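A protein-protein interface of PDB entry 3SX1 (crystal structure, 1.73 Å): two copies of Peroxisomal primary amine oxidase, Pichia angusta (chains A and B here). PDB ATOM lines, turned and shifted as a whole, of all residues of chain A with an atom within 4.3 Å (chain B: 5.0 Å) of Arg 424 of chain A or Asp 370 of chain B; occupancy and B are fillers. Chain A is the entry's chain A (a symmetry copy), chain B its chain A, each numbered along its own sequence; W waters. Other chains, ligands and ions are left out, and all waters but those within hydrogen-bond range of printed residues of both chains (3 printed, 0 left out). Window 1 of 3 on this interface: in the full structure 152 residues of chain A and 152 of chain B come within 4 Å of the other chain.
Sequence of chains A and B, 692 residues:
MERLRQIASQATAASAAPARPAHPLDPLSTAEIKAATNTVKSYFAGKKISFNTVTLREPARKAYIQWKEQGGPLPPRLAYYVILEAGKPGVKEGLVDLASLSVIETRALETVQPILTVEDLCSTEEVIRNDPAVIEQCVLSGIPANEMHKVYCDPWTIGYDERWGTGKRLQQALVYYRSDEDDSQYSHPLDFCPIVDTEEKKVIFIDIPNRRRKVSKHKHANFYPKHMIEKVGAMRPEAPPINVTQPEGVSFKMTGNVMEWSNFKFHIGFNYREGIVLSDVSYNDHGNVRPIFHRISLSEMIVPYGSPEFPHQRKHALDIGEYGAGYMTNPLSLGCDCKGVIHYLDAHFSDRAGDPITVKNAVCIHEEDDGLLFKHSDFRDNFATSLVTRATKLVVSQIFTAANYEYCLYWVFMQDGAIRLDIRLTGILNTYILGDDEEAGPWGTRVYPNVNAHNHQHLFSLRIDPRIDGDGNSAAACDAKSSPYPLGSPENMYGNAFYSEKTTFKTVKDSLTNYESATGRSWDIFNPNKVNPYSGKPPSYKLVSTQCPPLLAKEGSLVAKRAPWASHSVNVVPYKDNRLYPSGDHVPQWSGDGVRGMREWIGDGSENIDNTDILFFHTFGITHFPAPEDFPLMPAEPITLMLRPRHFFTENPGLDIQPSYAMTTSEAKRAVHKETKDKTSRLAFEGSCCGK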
ATOM      1  N   GLU A 406      20.724  -4.927   6.694  1.00  0.00           N
ATOM      2  CA  GLU A 406      19.612  -5.383   7.515  1.00  0.00           C
ATOM      3  C   GLU A 406      19.696  -6.901   7.593  1.00  0.00           C
ATOM      4  O   GLU A 406      19.879  -7.581   6.568  1.00  0.00           O
ATOM      5  CB  GLU A 406      18.272  -5.038   6.836  1.00  0.00           C
ATOM      6  CG  GLU A 406      17.577  -3.805   7.430  1.00  0.00           C
ATOM      7  CD  GLU A 406      18.152  -2.454   6.963  1.00  0.00           C
ATOM      8  OE1 GLU A 406      17.693  -1.430   7.526  1.00  0.00           O
ATOM      9  OE2 GLU A 406      18.954  -2.399   5.974  1.00  0.00           O
ATOM     10  N   TYR A 407      19.547  -7.414   8.796  1.00  0.00           N
ATOM     11  CA  TYR A 407      19.559  -8.864   9.038  1.00  0.00           C
ATOM     12  C   TYR A 407      18.205  -9.273   9.580  1.00  0.00           C
ATOM     13  O   TYR A 407      17.800  -8.855  10.676  1.00  0.00           O
ATOM     14  CB  TYR A 407      20.652  -9.217  10.079  1.00  0.00           C
ATOM     15  CG  TYR A 407      22.046  -8.977   9.562  1.00  0.00           C
ATOM     16  CD1 TYR A 407      22.648  -7.719   9.681  1.00  0.00           C
ATOM     17  CD2 TYR A 407      22.757 -10.013   8.954  1.00  0.00           C
ATOM     18  CE1 TYR A 407      23.939  -7.486   9.180  1.00  0.00           C
ATOM     19  CE2 TYR A 407      24.062  -9.804   8.488  1.00  0.00           C
ATOM     20  CZ  TYR A 407      24.623  -8.542   8.611  1.00  0.00           C
ATOM     21  OH  TYR A 407      25.906  -8.358   8.171  1.00  0.00           O
ATOM     22  N   CYS A 408      17.506 -10.087   8.797  1.00  0.00           N
ATOM     23  CA  CYS A 408      16.197 -10.600   9.162  1.00  0.00           C
ATOM     24  C   CYS A 408      16.380 -12.016   9.701  1.00  0.00           C
ATOM     25  O   CYS A 408      16.930 -12.870   8.993  1.00  0.00           O
ATOM     26  CB  CYS A 408      15.293 -10.636   7.936  1.00  0.00           C
ATOM     27  SG  CYS A 408      15.336  -9.055   7.005  1.00  0.00           S
ATOM     28  N   TYR A 410      14.797 -15.463  11.509  1.00  0.00           N
ATOM     29  CA  TYR A 410      13.559 -16.227  11.683  1.00  0.00           C
ATOM     30  C   TYR A 410      13.875 -17.552  12.356  1.00  0.00           C
ATOM     31  O   TYR A 410      14.507 -18.414  11.743  1.00  0.00           O
ATOM     32  CB  TYR A 410      12.911 -16.534  10.332  1.00  0.00           C
ATOM     33  CG  TYR A 410      12.694 -15.295   9.482  1.00  0.00           C
ATOM     34  CD1 TYR A 410      13.697 -14.838   8.639  1.00  0.00           C
ATOM     35  CD2 TYR A 410      11.503 -14.563   9.556  1.00  0.00           C
ATOM     36  CE1 TYR A 410      13.491 -13.712   7.827  1.00  0.00           C
ATOM     37  CE2 TYR A 410      11.284 -13.443   8.745  1.00  0.00           C
ATOM     38  CZ  TYR A 410      12.279 -13.027   7.879  1.00  0.00           C
ATOM     39  OH  TYR A 410      12.111 -11.852   7.126  1.00  0.00           O
ATOM     40  N   ILE A 423      17.877 -16.914   7.796  1.00  0.00           N
ATOM     41  CA  ILE A 423      18.281 -15.532   7.844  1.00  0.00           C
ATOM     42  C   ILE A 423      18.087 -14.975   6.417  1.00  0.00           C
ATOM     43  O   ILE A 423      18.288 -15.695   5.437  1.00  0.00           O
ATOM     44  CB  ILE A 423      19.759 -15.427   8.246  1.00  0.00           C
ATOM     45  CG1 ILE A 423      19.912 -15.861   9.721  1.00  0.00           C
ATOM     46  CG2 ILE A 423      20.235 -13.969   8.033  1.00  0.00           C
ATOM     47  CD1 ILE A 423      21.373 -15.853  10.238  1.00  0.00           C
ATOM     48  N   ARG A 424      17.617 -13.728   6.308  1.00  0.00           N
ATOM     49  CA  ARG A 424      17.622 -13.015   5.017  1.00  0.00           C
ATOM     50  C   ARG A 424      18.415 -11.719   5.201  1.00  0.00           C
ATOM     51  O   ARG A 424      18.175 -10.972   6.126  1.00  0.00           O
ATOM     52  CB  ARG A 424      16.198 -12.680   4.593  1.00  0.00           C
ATOM     53  CG  ARG A 424      15.429 -13.969   4.140  1.00  0.00           C
ATOM     54  CD  ARG A 424      14.170 -13.561   3.396  1.00  0.00           C
ATOM     55  NE  ARG A 424      13.345 -14.736   3.095  1.00  0.00           N
ATOM     56  CZ  ARG A 424      12.286 -14.693   2.304  1.00  0.00           C
ATOM     57  NH1 ARG A 424      11.995 -13.550   1.663  1.00  0.00           N
ATOM     58  NH2 ARG A 424      11.536 -15.784   2.141  1.00  0.00           N
ATOM     59  N   LEU A 425      19.434 -11.547   4.374  1.00  0.00           N
ATOM     60  CA  LEU A 425      20.281 -10.359   4.374  1.00  0.00           C
ATOM     61  C   LEU A 425      19.726  -9.390   3.342  1.00  0.00           C
ATOM     62  O   LEU A 425      19.565  -9.771   2.188  1.00  0.00           O
ATOM     63  CB  LEU A 425      21.688 -10.776   3.923  1.00  0.00           C
ATOM     64  CG  LEU A 425      22.376 -11.798   4.819  1.00  0.00           C
ATOM     65  CD1 LEU A 425      23.855 -11.789   4.573  1.00  0.00           C
ATOM     66  CD2 LEU A 425      22.094 -11.485   6.280  1.00  0.00           C
ATOM     67  N   THR A 426      19.546  -8.129   3.725  1.00  0.00           N
ATOM     68  CA  THR A 426      19.143  -7.104   2.759  1.00  0.00           C
ATOM     69  C   THR A 426      19.756  -5.793   3.225  1.00  0.00           C
ATOM     70  O   THR A 426      20.764  -5.818   3.958  1.00  0.00           O
ATOM     71  CB  THR A 426      17.613  -7.084   2.550  1.00  0.00           C
ATOM     72  OG1 THR A 426      17.265  -6.108   1.556  1.00  0.00           O
ATOM     73  CG2 THR A 426      16.852  -6.769   3.836  1.00  0.00           C
ATOM     74  N   ALA A 636      16.915  -9.625  -0.977  1.00  0.00           N
ATOM     75  CA  ALA A 636      17.184 -10.543   0.147  1.00  0.00           C
ATOM     76  C   ALA A 636      18.019 -11.755  -0.266  1.00  0.00           C
ATOM     77  O   ALA A 636      17.759 -12.394  -1.297  1.00  0.00           O
ATOM     78  CB  ALA A 636      15.886 -11.002   0.768  1.00  0.00           C
ATOM     79  N   GLU A 637      19.040 -12.042   0.521  1.00  0.00           N
ATOM     80  CA  GLU A 637      19.915 -13.213   0.265  1.00  0.00           C
ATOM     81  C   GLU A 637      19.718 -14.197   1.412  1.00  0.00           C
ATOM     82  O   GLU A 637      19.862 -13.805   2.572  1.00  0.00           O
ATOM     83  CB  GLU A 637      21.404 -12.827   0.222  1.00  0.00           C
ATOM     84  CG  GLU A 637      22.217 -14.053  -0.209  1.00  0.00           C
ATOM     85  CD  GLU A 637      23.618 -13.759  -0.675  1.00  0.00           C
ATOM     86  OE1 GLU A 637      24.016 -12.565  -0.676  1.00  0.00           O
ATOM     87  OE2 GLU A 637      24.341 -14.756  -0.934  1.00  0.00           O
ATOM     88  N   GLU B 368       2.467 -16.861  -4.753  1.00  0.00           N
ATOM     89  CA  GLU B 368       2.423 -16.911  -3.291  1.00  0.00           C
ATOM     90  C   GLU B 368       3.220 -15.744  -2.718  1.00  0.00           C
ATOM     91  O   GLU B 368       4.219 -15.348  -3.290  1.00  0.00           O
ATOM     92  CB  GLU B 368       3.107 -18.174  -2.747  1.00  0.00           C
ATOM     93  CG  GLU B 368       2.395 -19.509  -2.892  1.00  0.00           C
ATOM     94  CD  GLU B 368       3.211 -20.625  -2.229  1.00  0.00           C
ATOM     95  OE1 GLU B 368       3.618 -20.459  -1.051  1.00  0.00           O
ATOM     96  OE2 GLU B 368       3.563 -21.596  -2.918  1.00  0.00           O
ATOM     97  N   ASP B 369       2.862 -15.320  -1.515  1.00  0.00           N
ATOM     98  CA  ASP B 369       3.711 -14.481  -0.659  1.00  0.00           C
ATOM     99  C   ASP B 369       5.068 -15.133  -0.480  1.00  0.00           C
ATOM    100  O   ASP B 369       5.139 -16.343  -0.209  1.00  0.00           O
ATOM    101  CB  ASP B 369       3.092 -14.387   0.740  1.00  0.00           C
ATOM    102  CG  ASP B 369       1.898 -13.466   0.796  1.00  0.00           C
ATOM    103  OD1 ASP B 369       1.781 -12.583  -0.082  1.00  0.00           O
ATOM    104  OD2 ASP B 369       1.106 -13.596   1.761  1.00  0.00           O
ATOM    105  N   ASP B 370       6.148 -14.372  -0.592  1.00  0.00           N
ATOM    106  CA  ASP B 370       7.453 -14.963  -0.333  1.00  0.00           C
ATOM    107  C   ASP B 370       8.336 -14.137   0.636  1.00  0.00           C
ATOM    108  O   ASP B 370       9.591 -14.185   0.566  1.00  0.00           O
ATOM    109  CB  ASP B 370       8.185 -15.281  -1.633  1.00  0.00           C
ATOM    110  CG  ASP B 370       9.288 -16.312  -1.435  1.00  0.00           C
ATOM    111  OD1 ASP B 370       9.198 -17.075  -0.446  1.00  0.00           O
ATOM    112  OD2 ASP B 370      10.266 -16.330  -2.206  1.00  0.00           O
ATOM    113  N   GLY B 371       7.680 -13.538   1.621  1.00  0.00           N
ATOM    114  CA  GLY B 371       8.379 -12.747   2.658  1.00  0.00           C
ATOM    115  C   GLY B 371       8.913 -11.458   2.062  1.00  0.00           C
ATOM    116  O   GLY B 371       8.252 -10.857   1.210  1.00  0.00           O
ATOM    117  N   LEU B 372      10.065 -10.991   2.566  1.00  0.00           N
ATOM    118  CA  LEU B 372      10.584  -9.683   2.180  1.00  0.00           C
ATOM    119  C   LEU B 372      11.405  -9.805   0.904  1.00  0.00           C
ATOM    120  O   LEU B 372      12.195 -10.743   0.743  1.00  0.00           O
ATOM    121  CB  LEU B 372      11.457  -9.091   3.298  1.00  0.00           C
ATOM    122  CG  LEU B 372      10.728  -8.726   4.587  1.00  0.00           C
ATOM    123  CD1 LEU B 372      11.706  -8.013   5.537  1.00  0.00           C
ATOM    124  CD2 LEU B 372       9.534  -7.848   4.295  1.00  0.00           C
ATOM    125  N   ALA B 391       8.000  -9.651  -1.271  1.00  0.00           N
ATOM    126  CA  ALA B 391       8.223 -10.518  -2.442  1.00  0.00           C
ATOM    127  C   ALA B 391       6.986 -11.347  -2.754  1.00  0.00           C
ATOM    128  O   ALA B 391       6.328 -11.861  -1.838  1.00  0.00           O
ATOM    129  CB  ALA B 391       9.407 -11.467  -2.162  1.00  0.00           C
ATOM    130  N   THR B 392       6.784 -11.622  -4.038  1.00  0.00           N
ATOM    131  CA  THR B 392       5.818 -12.613  -4.473  1.00  0.00           C
ATOM    132  C   THR B 392       6.591 -13.598  -5.334  1.00  0.00           C
ATOM    133  O   THR B 392       7.517 -13.184  -6.016  1.00  0.00           O
ATOM    134  CB  THR B 392       4.734 -11.967  -5.336  1.00  0.00           C
ATOM    135  OG1 THR B 392       4.069 -10.953  -4.564  1.00  0.00           O
ATOM    136  CG2 THR B 392       3.721 -12.996  -5.764  1.00  0.00           C
ATOM    137  N   LYS B 393       6.283 -14.897  -5.217  1.00  0.00           N
ATOM    138  CA  LYS B 393       6.902 -15.909  -6.104  1.00  0.00           C
ATOM    139  C   LYS B 393       5.852 -16.602  -6.953  1.00  0.00           C
ATOM    140  O   LYS B 393       4.661 -16.692  -6.558  1.00  0.00           O
ATOM    141  CB  LYS B 393       7.662 -16.940  -5.279  1.00  0.00           C
ATOM    142  CG  LYS B 393       6.774 -17.759  -4.384  1.00  0.00           C
ATOM    143  CD  LYS B 393       7.618 -18.711  -3.579  1.00  0.00           C
ATOM    144  CE  LYS B 393       6.740 -19.329  -2.479  1.00  0.00           C
ATOM    145  NZ  LYS B 393       7.516 -20.329  -1.699  1.00  0.00           N
ATOM    146  N   MET B 414      11.226 -15.661  -9.191  1.00  0.00           N
ATOM    147  CA  MET B 414      11.228 -14.668  -8.131  1.00  0.00           C
ATOM    148  C   MET B 414      11.502 -13.279  -8.677  1.00  0.00           C
ATOM    149  O   MET B 414      11.932 -13.096  -9.826  1.00  0.00           O
ATOM    150  CB  MET B 414      12.180 -15.055  -6.983  1.00  0.00           C
ATOM    151  CG  MET B 414      11.627 -16.162  -6.050  1.00  0.00           C
ATOM    152  SD  MET B 414      12.963 -16.916  -5.129  1.00  0.00           S
ATOM    153  CE  MET B 414      13.873 -17.487  -6.562  1.00  0.00           C
ATOM    154  N   ARG B 420      14.414 -20.773  -9.023  1.00  0.00           N
ATOM    155  CA  ARG B 420      14.831 -21.791  -8.062  1.00  0.00           C
ATOM    156  C   ARG B 420      14.070 -23.061  -8.380  1.00  0.00           C
ATOM    157  O   ARG B 420      12.935 -23.012  -8.874  1.00  0.00           O
ATOM    158  CB  ARG B 420      14.460 -21.270  -6.665  1.00  0.00           C
ATOM    159  CG  ARG B 420      14.880 -22.107  -5.518  1.00  0.00           C
ATOM    160  CD  ARG B 420      14.567 -21.295  -4.237  1.00  0.00           C
ATOM    161  NE  ARG B 420      13.163 -21.376  -3.885  1.00  0.00           N
ATOM    162  CZ  ARG B 420      12.532 -20.497  -3.110  1.00  0.00           C
ATOM    163  NH1 ARG B 420      13.189 -19.433  -2.650  1.00  0.00           N
ATOM    164  NH2 ARG B 420      11.252 -20.671  -2.785  1.00  0.00           N
HETATM  165  O   HOH W   1       8.628 -17.433   2.382  1.00  0.00           O
HETATM  166  O   HOH W   2      13.134 -12.523  -1.456  1.00  0.00           O
HETATM  167  O   HOH W   3      11.230 -12.683   4.733  1.00  0.00           O
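NH2 of Arg 424 of chain A is in salt-bridge range of OD1 of Asp 370 of chain B (3.7 Å).
O of Leu 372 of chain B lies within hydrogen-bond range of NH1 of Arg 424 of chain A.
The backbone NH of Asp 370 of chain B is in hydrogen-bond range of the backbone carbonyl oxygen of Ala 391 of chain B.
The side-chain carboxylate of Asp 370 of chain B lies within salt-bridge range of the side-chain amino group of Lys 393 of chain B (3.9 Å).
The backbone carbonyl oxygen (O) of Gly 371 of chain B is in hydrogen-bond range of the backbone NH (N) of Ala 391 of chain B (2.8 Å).
O of Arg 424 of chain A is in hydrogen-bond range of N of Cys 408 of chain A.
Arg 424 of chain A touches Gly 371 of chain B.
Leu 372 of chain B touches Ala 636 of chain A (O to CB, 3.7 Å).
Printed residues of chain B within 4 Å of Arg 424 of chain A: Asp 370 (2.7 Å), Gly 371 (3.7 Å) and Leu 372 (3.0 Å).
Leu 425 of chain A touches none of the printed residues of chain B.
Of the printed residues of chain B, Ala 636 of chain A touches Leu 372 (3.7 Å).
Of the printed residues of chain A, Gly 371 of chain B touches Arg 424.
Of the printed residues of chain A, Leu 372 of chain B touches Arg 424 and Ala 636.
The nearest printed residue of chain A that does not touch Asp 370 of chain B is Ala 636 of chain A (7.1 Å).
The nearest printed residue of chain B that does not touch Ala 636 of chain A is Asp 370 of chain B (7.1 Å).
No position is printed for both chains.
Of the 4 pairs that touch across the chains among the printed residues, none has its exchanged pair printed and touching as well.
Printed residues of chain B that touch a printed residue of chain A: Asp 370, Gly 371 and Leu 372.
Of the 10 printed residues of chain A, 2 touch a printed residue of chain B.
Among the printed residues, Asp or Glu carboxylates within 4 Å of a Lys or Arg side-chain nitrogen of the other chain: Arg 424 of chain A with Asp 370 of chain B.
Water W3 lies within hydrogen-bond range of OH of Tyr 410 of chain A (2.7 Å), N of Leu 372 of chain B (3.0 Å) and NH1 of Arg 424 of chain A (3.3 Å).
Water W1 lies within hydrogen-bond range of OD1 of Asp 370 of chain B (2.9 Å) and NH2 of Arg 424 of chain A (3.4 Å).
Water W2 bridges O of Leu 372 of chain B (3.0 Å) and NH1 of Arg 424 of chain A (3.5 Å).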
